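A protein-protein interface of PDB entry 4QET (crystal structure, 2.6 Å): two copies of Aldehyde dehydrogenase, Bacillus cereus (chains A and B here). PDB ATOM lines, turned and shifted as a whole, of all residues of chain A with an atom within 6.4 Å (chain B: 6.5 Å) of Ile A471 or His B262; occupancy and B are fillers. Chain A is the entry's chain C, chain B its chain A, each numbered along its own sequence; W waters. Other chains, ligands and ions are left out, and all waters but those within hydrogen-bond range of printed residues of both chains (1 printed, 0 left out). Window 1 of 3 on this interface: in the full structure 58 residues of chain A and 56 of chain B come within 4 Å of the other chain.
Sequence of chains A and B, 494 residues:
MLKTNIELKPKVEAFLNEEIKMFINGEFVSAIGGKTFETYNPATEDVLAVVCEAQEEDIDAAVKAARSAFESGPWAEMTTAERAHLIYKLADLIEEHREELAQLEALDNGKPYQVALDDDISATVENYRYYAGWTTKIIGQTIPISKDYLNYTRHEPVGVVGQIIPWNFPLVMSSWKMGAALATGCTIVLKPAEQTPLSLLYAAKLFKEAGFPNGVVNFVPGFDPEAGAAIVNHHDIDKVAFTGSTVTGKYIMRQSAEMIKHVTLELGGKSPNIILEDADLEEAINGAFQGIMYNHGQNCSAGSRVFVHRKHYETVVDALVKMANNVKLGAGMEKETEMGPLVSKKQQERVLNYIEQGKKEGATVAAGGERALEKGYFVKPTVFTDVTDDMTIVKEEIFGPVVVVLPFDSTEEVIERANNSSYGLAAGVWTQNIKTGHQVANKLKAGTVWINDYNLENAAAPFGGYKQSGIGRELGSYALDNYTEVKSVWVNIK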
ATOM      1  N   MET A 253      14.756 -33.234 -19.181  1.00  0.00           N
ATOM      2  CA  MET A 253      13.560 -32.668 -19.741  1.00  0.00           C
ATOM      3  C   MET A 253      12.700 -33.780 -20.331  1.00  0.00           C
ATOM      4  O   MET A 253      11.487 -33.798 -20.117  1.00  0.00           O
ATOM      5  CB  MET A 253      13.865 -31.606 -20.783  1.00  0.00           C
ATOM      6  CG  MET A 253      12.660 -30.731 -21.080  1.00  0.00           C
ATOM      7  SD  MET A 253      13.099 -29.332 -22.119  1.00  0.00           S
ATOM      8  CE  MET A 253      11.431 -28.689 -22.370  1.00  0.00           C
ATOM      9  N   HIS A 262       7.031 -29.167 -14.557  1.00  0.00           N
ATOM     10  CA  HIS A 262       7.824 -27.978 -14.820  1.00  0.00           C
ATOM     11  C   HIS A 262       9.321 -28.310 -14.633  1.00  0.00           C
ATOM     12  O   HIS A 262       9.741 -28.964 -13.666  1.00  0.00           O
ATOM     13  CB  HIS A 262       7.404 -26.816 -13.896  1.00  0.00           C
ATOM     14  CG  HIS A 262       8.122 -25.523 -14.175  1.00  0.00           C
ATOM     15  ND1 HIS A 262       7.585 -24.523 -14.958  1.00  0.00           N
ATOM     16  CD2 HIS A 262       9.345 -25.080 -13.782  1.00  0.00           C
ATOM     17  CE1 HIS A 262       8.448 -23.523 -15.040  1.00  0.00           C
ATOM     18  NE2 HIS A 262       9.527 -23.839 -14.340  1.00  0.00           N
ATOM     19  N   VAL A 263      10.131 -27.847 -15.563  1.00  0.00           N
ATOM     20  CA  VAL A 263      11.562 -28.055 -15.474  1.00  0.00           C
ATOM     21  C   VAL A 263      12.252 -26.710 -15.457  1.00  0.00           C
ATOM     22  O   VAL A 263      11.814 -25.771 -16.132  1.00  0.00           O
ATOM     23  CB  VAL A 263      12.101 -28.856 -16.678  1.00  0.00           C
ATOM     24  CG1 VAL A 263      13.571 -29.136 -16.479  1.00  0.00           C
ATOM     25  CG2 VAL A 263      11.379 -30.183 -16.828  1.00  0.00           C
ATOM     26  N   THR A 264      13.317 -26.585 -14.677  1.00  0.00           N
ATOM     27  CA  THR A 264      14.189 -25.444 -14.889  1.00  0.00           C
ATOM     28  C   THR A 264      15.608 -25.971 -15.036  1.00  0.00           C
ATOM     29  O   THR A 264      16.042 -26.827 -14.266  1.00  0.00           O
ATOM     30  CB  THR A 264      13.926 -24.305 -13.887  1.00  0.00           C
ATOM     31  OG1 THR A 264      15.106 -23.560 -13.680  1.00  0.00           O
ATOM     32  CG2 THR A 264      13.526 -24.805 -12.625  1.00  0.00           C
ATOM     33  N   LEU A 265      16.277 -25.523 -16.099  1.00  0.00           N
ATOM     34  CA  LEU A 265      17.578 -26.050 -16.540  1.00  0.00           C
ATOM     35  C   LEU A 265      18.583 -24.967 -16.673  1.00  0.00           C
ATOM     36  O   LEU A 265      18.307 -23.984 -17.361  1.00  0.00           O
ATOM     37  CB  LEU A 265      17.468 -26.659 -17.932  1.00  0.00           C
ATOM     38  CG  LEU A 265      16.424 -27.759 -18.027  1.00  0.00           C
ATOM     39  CD1 LEU A 265      16.181 -28.123 -19.496  1.00  0.00           C
ATOM     40  CD2 LEU A 265      16.848 -28.943 -17.158  1.00  0.00           C
ATOM     41  N   GLU A 266      19.753 -25.178 -16.062  1.00  0.00           N
ATOM     42  CA  GLU A 266      20.876 -24.235 -16.122  1.00  0.00           C
ATOM     43  C   GLU A 266      22.082 -24.988 -16.694  1.00  0.00           C
ATOM     44  O   GLU A 266      22.639 -25.878 -16.022  1.00  0.00           O
ATOM     45  CB  GLU A 266      21.178 -23.708 -14.706  1.00  0.00           C
ATOM     46  CG  GLU A 266      21.868 -22.369 -14.667  1.00  0.00           C
ATOM     47  CD  GLU A 266      20.879 -21.251 -14.873  1.00  0.00           C
ATOM     48  OE1 GLU A 266      21.110 -20.420 -15.765  1.00  0.00           O
ATOM     49  OE2 GLU A 266      19.852 -21.208 -14.171  1.00  0.00           O
ATOM     50  N   LEU A 267      22.479 -24.677 -17.935  1.00  0.00           N
ATOM     51  CA  LEU A 267      23.389 -25.577 -18.662  1.00  0.00           C
ATOM     52  C   LEU A 267      24.658 -24.872 -19.125  1.00  0.00           C
ATOM     53  O   LEU A 267      25.034 -23.823 -18.566  1.00  0.00           O
ATOM     54  CB  LEU A 267      22.679 -26.238 -19.858  1.00  0.00           C
ATOM     55  CG  LEU A 267      21.238 -26.745 -19.756  1.00  0.00           C
ATOM     56  CD1 LEU A 267      20.798 -27.342 -21.080  1.00  0.00           C
ATOM     57  CD2 LEU A 267      21.084 -27.755 -18.615  1.00  0.00           C
ATOM     58  N   GLY A 465      20.229 -19.170 -19.490  1.00  0.00           N
ATOM     59  CA  GLY A 465      20.641 -19.119 -20.872  1.00  0.00           C
ATOM     60  C   GLY A 465      19.521 -19.047 -21.900  1.00  0.00           C
ATOM     61  O   GLY A 465      18.415 -19.565 -21.668  1.00  0.00           O
ATOM     62  N   LYS A 467      18.657 -20.229 -25.991  1.00  0.00           N
ATOM     63  CA  LYS A 467      18.948 -21.420 -26.759  1.00  0.00           C
ATOM     64  C   LYS A 467      19.227 -22.645 -25.848  1.00  0.00           C
ATOM     65  O   LYS A 467      18.439 -22.920 -24.905  1.00  0.00           O
ATOM     66  CB  LYS A 467      20.109 -21.164 -27.720  1.00  0.00           C
ATOM     67  CG  LYS A 467      19.971 -19.923 -28.606  1.00  0.00           C
ATOM     68  CD  LYS A 467      21.335 -19.368 -28.963  1.00  0.00           C
ATOM     69  CE  LYS A 467      21.294 -18.753 -30.333  1.00  0.00           C
ATOM     70  NZ  LYS A 467      22.624 -18.176 -30.664  1.00  0.00           N
ATOM     71  N   SER A 469      21.593 -23.103 -23.723  1.00  0.00           N
ATOM     72  CA  SER A 469      22.174 -22.819 -22.410  1.00  0.00           C
ATOM     73  C   SER A 469      21.226 -23.001 -21.192  1.00  0.00           C
ATOM     74  O   SER A 469      21.679 -23.022 -20.046  1.00  0.00           O
ATOM     75  CB  SER A 469      22.857 -21.466 -22.418  1.00  0.00           C
ATOM     76  OG  SER A 469      24.020 -21.556 -23.217  1.00  0.00           O
ATOM     77  N   GLY A 470      19.925 -23.162 -21.457  1.00  0.00           N
ATOM     78  CA  GLY A 470      18.956 -23.545 -20.422  1.00  0.00           C
ATOM     79  C   GLY A 470      17.515 -23.125 -20.716  1.00  0.00           C
ATOM     80  O   GLY A 470      17.213 -22.650 -21.821  1.00  0.00           O
ATOM     81  N   ILE A 471      16.641 -23.355 -19.726  1.00  0.00           N
ATOM     82  CA  ILE A 471      15.252 -22.873 -19.686  1.00  0.00           C
ATOM     83  C   ILE A 471      15.056 -22.246 -18.320  1.00  0.00           C
ATOM     84  O   ILE A 471      15.284 -22.903 -17.318  1.00  0.00           O
ATOM     85  CB  ILE A 471      14.229 -24.030 -19.873  1.00  0.00           C
ATOM     86  CG1 ILE A 471      14.277 -24.491 -21.322  1.00  0.00           C
ATOM     87  CG2 ILE A 471      12.791 -23.610 -19.508  1.00  0.00           C
ATOM     88  CD1 ILE A 471      13.490 -25.749 -21.575  1.00  0.00           C
ATOM     89  N   GLY A 472      14.628 -20.987 -18.276  1.00  0.00           N
ATOM     90  CA  GLY A 472      14.348 -20.330 -17.018  1.00  0.00           C
ATOM     91  C   GLY A 472      15.525 -19.576 -16.439  1.00  0.00           C
ATOM     92  O   GLY A 472      16.670 -19.644 -16.935  1.00  0.00           O
ATOM     93  N   ARG A 473      15.234 -18.824 -15.381  1.00  0.00           N
ATOM     94  CA  ARG A 473      16.236 -18.040 -14.731  1.00  0.00           C
ATOM     95  C   ARG A 473      16.340 -18.455 -13.274  1.00  0.00           C
ATOM     96  O   ARG A 473      15.370 -18.930 -12.718  1.00  0.00           O
ATOM     97  CB  ARG A 473      15.879 -16.561 -14.866  1.00  0.00           C
ATOM     98  CG  ARG A 473      15.916 -16.117 -16.309  1.00  0.00           C
ATOM     99  CD  ARG A 473      17.361 -16.111 -16.826  1.00  0.00           C
ATOM    100  NE  ARG A 473      17.439 -15.590 -18.188  1.00  0.00           N
ATOM    101  CZ  ARG A 473      17.294 -16.327 -19.282  1.00  0.00           C
ATOM    102  NH1 ARG A 473      17.088 -17.635 -19.166  1.00  0.00           N
ATOM    103  NH2 ARG A 473      17.365 -15.753 -20.480  1.00  0.00           N
ATOM    104  N   ASN A 482       9.694 -20.058 -10.875  1.00  0.00           N
ATOM    105  CA  ASN A 482       9.896 -21.453 -11.123  1.00  0.00           C
ATOM    106  C   ASN A 482       9.302 -22.327 -10.051  1.00  0.00           C
ATOM    107  O   ASN A 482       9.053 -23.498 -10.333  1.00  0.00           O
ATOM    108  CB  ASN A 482      11.382 -21.792 -11.226  1.00  0.00           C
ATOM    109  CG  ASN A 482      12.130 -20.894 -12.192  1.00  0.00           C
ATOM    110  OD1 ASN A 482      13.266 -20.472 -11.908  1.00  0.00           O
ATOM    111  ND2 ASN A 482      11.514 -20.606 -13.334  1.00  0.00           N
ATOM    112  N   VAL B 158      11.352 -13.966 -27.581  1.00  0.00           N
ATOM    113  CA  VAL B 158      12.156 -15.189 -27.746  1.00  0.00           C
ATOM    114  C   VAL B 158      12.561 -15.484 -29.191  1.00  0.00           C
ATOM    115  O   VAL B 158      13.557 -16.156 -29.396  1.00  0.00           O
ATOM    116  CB  VAL B 158      11.477 -16.439 -27.143  1.00  0.00           C
ATOM    117  CG1 VAL B 158      10.237 -16.802 -27.920  1.00  0.00           C
ATOM    118  CG2 VAL B 158      12.439 -17.631 -27.120  1.00  0.00           C
ATOM    119  N   ASP B 238      12.288 -21.266 -31.912  1.00  0.00           N
ATOM    120  CA  ASP B 238      12.867 -20.956 -30.617  1.00  0.00           C
ATOM    121  C   ASP B 238      12.097 -21.487 -29.399  1.00  0.00           C
ATOM    122  O   ASP B 238      12.670 -21.689 -28.344  1.00  0.00           O
ATOM    123  CB  ASP B 238      13.086 -19.456 -30.503  1.00  0.00           C
ATOM    124  CG  ASP B 238      14.099 -18.973 -31.499  1.00  0.00           C
ATOM    125  OD1 ASP B 238      15.255 -19.385 -31.348  1.00  0.00           O
ATOM    126  OD2 ASP B 238      13.739 -18.222 -32.449  1.00  0.00           O
ATOM    127  N   LYS B 239      10.804 -21.736 -29.566  1.00  0.00           N
ATOM    128  CA  LYS B 239       9.929 -21.982 -28.455  1.00  0.00           C
ATOM    129  C   LYS B 239       8.640 -22.552 -29.036  1.00  0.00           C
ATOM    130  O   LYS B 239       8.243 -22.247 -30.187  1.00  0.00           O
ATOM    131  CB  LYS B 239       9.691 -20.672 -27.690  1.00  0.00           C
ATOM    132  CG  LYS B 239       8.844 -20.710 -26.428  1.00  0.00           C
ATOM    133  CD  LYS B 239       7.320 -20.600 -26.698  1.00  0.00           C
ATOM    134  CE  LYS B 239       6.447 -20.657 -25.418  1.00  0.00           C
ATOM    135  NZ  LYS B 239       6.476 -21.961 -24.704  1.00  0.00           N
ATOM    136  N   VAL B 240       7.991 -23.394 -28.222  1.00  0.00           N
ATOM    137  CA  VAL B 240       6.815 -24.091 -28.684  1.00  0.00           C
ATOM    138  C   VAL B 240       5.688 -24.006 -27.659  1.00  0.00           C
ATOM    139  O   VAL B 240       5.902 -24.091 -26.451  1.00  0.00           O
ATOM    140  CB  VAL B 240       7.151 -25.549 -29.151  1.00  0.00           C
ATOM    141  CG1 VAL B 240       7.558 -26.415 -27.981  1.00  0.00           C
ATOM    142  CG2 VAL B 240       5.966 -26.214 -29.830  1.00  0.00           C
ATOM    143  N   ALA B 241       4.486 -23.835 -28.190  1.00  0.00           N
ATOM    144  CA  ALA B 241       3.290 -23.830 -27.414  1.00  0.00           C
ATOM    145  C   ALA B 241       2.238 -24.708 -28.049  1.00  0.00           C
ATOM    146  O   ALA B 241       1.975 -24.621 -29.249  1.00  0.00           O
ATOM    147  CB  ALA B 241       2.769 -22.400 -27.273  1.00  0.00           C
ATOM    148  N   SER B 256      10.717 -31.482 -27.664  1.00  0.00           N
ATOM    149  CA  SER B 256      11.230 -30.187 -27.323  1.00  0.00           C
ATOM    150  C   SER B 256      12.521 -30.294 -26.539  1.00  0.00           C
ATOM    151  O   SER B 256      13.422 -29.480 -26.751  1.00  0.00           O
ATOM    152  CB  SER B 256      10.207 -29.414 -26.528  1.00  0.00           C
ATOM    153  OG  SER B 256       9.187 -28.951 -27.396  1.00  0.00           O
ATOM    154  N   MET B 259      16.181 -29.926 -28.045  1.00  0.00           N
ATOM    155  CA  MET B 259      16.766 -28.624 -28.309  1.00  0.00           C
ATOM    156  C   MET B 259      16.701 -27.601 -27.179  1.00  0.00           C
ATOM    157  O   MET B 259      16.954 -26.440 -27.410  1.00  0.00           O
ATOM    158  CB  MET B 259      16.171 -28.039 -29.580  1.00  0.00           C
ATOM    159  CG  MET B 259      16.730 -28.702 -30.841  1.00  0.00           C
ATOM    160  SD  MET B 259      15.413 -28.702 -32.043  1.00  0.00           S
ATOM    161  CE  MET B 259      14.092 -29.581 -31.156  1.00  0.00           C
ATOM    162  N   ILE B 260      16.416 -28.038 -25.955  1.00  0.00           N
ATOM    163  CA  ILE B 260      16.148 -27.133 -24.804  1.00  0.00           C
ATOM    164  C   ILE B 260      15.220 -25.947 -25.194  1.00  0.00           C
ATOM    165  O   ILE B 260      15.505 -24.738 -24.901  1.00  0.00           O
ATOM    166  CB  ILE B 260      17.451 -26.720 -24.054  1.00  0.00           C
ATOM    167  CG1 ILE B 260      18.235 -27.963 -23.670  1.00  0.00           C
ATOM    168  CG2 ILE B 260      17.154 -26.035 -22.729  1.00  0.00           C
ATOM    169  CD1 ILE B 260      19.429 -28.133 -24.542  1.00  0.00           C
ATOM    170  N   LYS B 261      14.131 -26.332 -25.886  1.00  0.00           N
ATOM    171  CA  LYS B 261      13.026 -25.465 -26.287  1.00  0.00           C
ATOM    172  C   LYS B 261      12.048 -25.290 -25.106  1.00  0.00           C
ATOM    173  O   LYS B 261      11.569 -26.274 -24.522  1.00  0.00           O
ATOM    174  CB  LYS B 261      12.299 -26.109 -27.459  1.00  0.00           C
ATOM    175  CG  LYS B 261      11.902 -25.188 -28.591  1.00  0.00           C
ATOM    176  CD  LYS B 261      11.531 -25.992 -29.832  1.00  0.00           C
ATOM    177  CE  LYS B 261      12.732 -26.334 -30.702  1.00  0.00           C
ATOM    178  NZ  LYS B 261      12.330 -26.606 -32.110  1.00  0.00           N
ATOM    179  N   HIS B 262      11.793 -24.036 -24.730  1.00  0.00           N
ATOM    180  CA  HIS B 262      10.752 -23.713 -23.761  1.00  0.00           C
ATOM    181  C   HIS B 262       9.400 -24.293 -24.243  1.00  0.00           C
ATOM    182  O   HIS B 262       9.004 -24.132 -25.416  1.00  0.00           O
ATOM    183  CB  HIS B 262      10.694 -22.187 -23.562  1.00  0.00           C
ATOM    184  CG  HIS B 262       9.720 -21.736 -22.510  1.00  0.00           C
ATOM    185  ND1 HIS B 262      10.092 -21.479 -21.206  1.00  0.00           N
ATOM    186  CD2 HIS B 262       8.384 -21.505 -22.568  1.00  0.00           C
ATOM    187  CE1 HIS B 262       9.034 -21.092 -20.514  1.00  0.00           C
ATOM    188  NE2 HIS B 262       7.989 -21.101 -21.320  1.00  0.00           N
ATOM    189  N   VAL B 263       8.701 -24.967 -23.340  1.00  0.00           N
ATOM    190  CA  VAL B 263       7.351 -25.464 -23.604  1.00  0.00           C
ATOM    191  C   VAL B 263       6.248 -24.790 -22.763  1.00  0.00           C
ATOM    192  O   VAL B 263       6.388 -24.578 -21.532  1.00  0.00           O
ATOM    193  CB  VAL B 263       7.303 -26.994 -23.382  1.00  0.00           C
ATOM    194  CG1 VAL B 263       5.933 -27.453 -22.935  1.00  0.00           C
ATOM    195  CG2 VAL B 263       7.696 -27.724 -24.643  1.00  0.00           C
ATOM    196  N   THR B 264       5.151 -24.473 -23.437  1.00  0.00           N
ATOM    197  CA  THR B 264       3.919 -24.103 -22.758  1.00  0.00           C
ATOM    198  C   THR B 264       2.846 -25.118 -23.166  1.00  0.00           C
ATOM    199  O   THR B 264       2.608 -25.316 -24.361  1.00  0.00           O
ATOM    200  CB  THR B 264       3.467 -22.666 -23.087  1.00  0.00           C
ATOM    201  OG1 THR B 264       4.532 -21.744 -22.818  1.00  0.00           O
ATOM    202  CG2 THR B 264       2.300 -22.280 -22.193  1.00  0.00           C
ATOM    203  N   ILE B 471       1.786 -27.081 -18.284  1.00  0.00           N
ATOM    204  CA  ILE B 471       2.895 -26.254 -17.816  1.00  0.00           C
ATOM    205  C   ILE B 471       2.681 -24.832 -18.391  1.00  0.00           C
ATOM    206  O   ILE B 471       2.435 -24.669 -19.618  1.00  0.00           O
ATOM    207  CB  ILE B 471       4.284 -26.768 -18.281  1.00  0.00           C
ATOM    208  CG1 ILE B 471       4.646 -28.050 -17.542  1.00  0.00           C
ATOM    209  CG2 ILE B 471       5.380 -25.724 -18.031  1.00  0.00           C
ATOM    210  CD1 ILE B 471       5.653 -28.897 -18.267  1.00  0.00           C
ATOM    211  N   GLY B 472       2.780 -23.827 -17.512  1.00  0.00           N
ATOM    212  CA  GLY B 472       2.686 -22.414 -17.874  1.00  0.00           C
ATOM    213  C   GLY B 472       1.253 -21.911 -17.787  1.00  0.00           C
ATOM    214  O   GLY B 472       0.319 -22.699 -17.571  1.00  0.00           O
ATOM    215  N   ASP B 481       5.462 -13.914 -20.344  1.00  0.00           N
ATOM    216  CA  ASP B 481       6.685 -14.514 -19.881  1.00  0.00           C
ATOM    217  C   ASP B 481       7.070 -15.713 -20.689  1.00  0.00           C
ATOM    218  O   ASP B 481       8.250 -16.083 -20.698  1.00  0.00           O
ATOM    219  CB  ASP B 481       6.550 -14.949 -18.420  1.00  0.00           C
ATOM    220  CG  ASP B 481       6.281 -13.767 -17.477  1.00  0.00           C
ATOM    221  OD1 ASP B 481       6.440 -12.600 -17.871  1.00  0.00           O
ATOM    222  OD2 ASP B 481       5.899 -14.011 -16.318  1.00  0.00           O
ATOM    223  N   ASN B 482       6.093 -16.354 -21.329  1.00  0.00           N
ATOM    224  CA  ASN B 482       6.422 -17.525 -22.147  1.00  0.00           C
ATOM    225  C   ASN B 482       7.097 -17.103 -23.445  1.00  0.00           C
ATOM    226  O   ASN B 482       7.803 -17.896 -24.046  1.00  0.00           O
ATOM    227  CB  ASN B 482       5.217 -18.392 -22.484  1.00  0.00           C
ATOM    228  CG  ASN B 482       4.480 -18.851 -21.265  1.00  0.00           C
ATOM    229  OD1 ASN B 482       3.246 -18.846 -21.232  1.00  0.00           O
ATOM    230  ND2 ASN B 482       5.215 -19.228 -20.254  1.00  0.00           N
ATOM    231  N   TYR B 483       6.891 -15.854 -23.854  1.00  0.00           N
ATOM    232  CA  TYR B 483       7.348 -15.452 -25.164  1.00  0.00           C
ATOM    233  C   TYR B 483       8.581 -14.561 -25.060  1.00  0.00           C
ATOM    234  O   TYR B 483       9.048 -13.994 -26.052  1.00  0.00           O
ATOM    235  CB  TYR B 483       6.194 -14.841 -25.989  1.00  0.00           C
ATOM    236  CG  TYR B 483       5.157 -15.886 -26.245  1.00  0.00           C
ATOM    237  CD1 TYR B 483       5.482 -17.002 -26.977  1.00  0.00           C
ATOM    238  CD2 TYR B 483       3.885 -15.813 -25.687  1.00  0.00           C
ATOM    239  CE1 TYR B 483       4.560 -18.009 -27.204  1.00  0.00           C
ATOM    240  CE2 TYR B 483       2.955 -16.808 -25.901  1.00  0.00           C
ATOM    241  CZ  TYR B 483       3.310 -17.911 -26.665  1.00  0.00           C
ATOM    242  OH  TYR B 483       2.426 -18.948 -26.911  1.00  0.00           O
ATOM    243  N   THR B 484       9.143 -14.522 -23.858  1.00  0.00           N
ATOM    244  CA  THR B 484      10.189 -13.595 -23.514  1.00  0.00           C
ATOM    245  C   THR B 484      11.440 -14.356 -23.128  1.00  0.00           C
ATOM    246  O   THR B 484      11.344 -15.415 -22.536  1.00  0.00           O
ATOM    247  CB  THR B 484       9.627 -12.690 -22.383  1.00  0.00           C
ATOM    248  OG1 THR B 484       9.193 -11.467 -22.975  1.00  0.00           O
ATOM    249  CG2 THR B 484      10.598 -12.403 -21.232  1.00  0.00           C
ATOM    250  N   GLU B 485      12.612 -13.860 -23.493  1.00  0.00           N
ATOM    251  CA  GLU B 485      13.868 -14.271 -22.813  1.00  0.00           C
ATOM    252  C   GLU B 485      14.308 -13.110 -21.973  1.00  0.00           C
ATOM    253  O   GLU B 485      14.319 -11.957 -22.463  1.00  0.00           O
ATOM    254  CB  GLU B 485      15.024 -14.587 -23.786  1.00  0.00           C
ATOM    255  CG  GLU B 485      14.901 -15.922 -24.501  1.00  0.00           C
ATOM    256  CD  GLU B 485      15.269 -17.102 -23.617  1.00  0.00           C
ATOM    257  OE1 GLU B 485      15.080 -18.245 -24.076  1.00  0.00           O
ATOM    258  OE2 GLU B 485      15.763 -16.892 -22.475  1.00  0.00           O
HETATM  259  O   HOH W   1      14.366 -16.048 -19.739  1.00  0.00           O
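The side-chain carboxylate (OE2) of Glu B485 is in salt-bridge range of the guanidinium group (NH2) of Arg A473, 2.8 Å away.
The backbone carbonyl oxygen of Lys A467 sits close to the backbone carbonyl oxygen of Ile B260 (3.5 Å).
O of His B262 is in hydrogen-bond range of N of Val B240 (3.1 Å).
N of Lys B261 lies within hydrogen-bond range of O of Ser B256, at 3.3 Å.
The side-chain amino group of Lys B261 lies close to the side-chain sulfur of Met B259, 3.7 Å away.
O of Leu A265 lies within hydrogen-bond range of N of Ile A471.
O of Ser A469 is in hydrogen-bond range of N of Leu A267.
NH1 of Arg A473 lies within hydrogen-bond range of O of Gly A465.
Hydrophobic or aromatic side chains of chain B that line the printed part of chain A: Ile B260, His B262 and Ile B471.
Of the 15 printed residues of chain A, 9 touch a printed residue of chain B.
Among the printed residues, Asp or Glu carboxylates within 4 Å of a Lys or Arg side-chain nitrogen of the other chain: Arg A473 with Glu B485 (2.8 Å).
Water W1 bridges the guanidinium group of Arg A473 (3.1 Å) and the side-chain carboxylate of Glu B485 (3.2 Å).
Of the printed residues of chain B, Met A253 touches Lys B261.
Printed residues of chain B within 4 Å of Gly A465: Glu B485.
Ile A471 touches just these residues of chain B: Ile B260 (3.6 Å), Lys B261 (3.6 Å) and His B262 (3.8 Å).
Lys B239 touches none of the printed residues of chain A.
Printed residues of chain A within 4 Å of Ile B260: Leu A265 (3.97 Å), Leu A267 (3.7 Å), Lys A467 (3.5 Å), Gly A470 (3.5 Å) and Ile A471 (3.6 Å).
Of the printed residues of chain A, His B262 touches Ile A471 (3.8 Å).
Of the printed residues of chain A, Ile B471 touches His A262.
The nearest residue of chain B that does not touch Ile A471 is Val B263 (5.2 Å).
The nearest printed residue of chain A that does not touch Ile B260 is Met A253 (4.6 Å).
Met A253 touches Lys B261.
Ile B471 touches His A262.
CG2 of Ile B260 touches CD1 of Leu A265 (3.97 Å).
CD1 of Leu A267 touches CG1 of Ile B260, 3.7 Å away.
O of Gly A465 touches OE2 of Glu B485 (3.9 Å).
Gly A470 touches Ile B260 (O to CG2, 3.5 Å).
Ile B260 touches Ile A471 (CG2 to CG1, 3.6 Å).
Ile A471 touches Lys B261.
Ile A471 touches His B262 (CG2 to ND1, 3.8 Å).
His A262 touches Ile B471, and with the chains exchanged Ile A471 touches His B262.
Of the 11 pairs that touch across the chains among the printed residues, 2 have their exchanged pair printed and touching as well.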
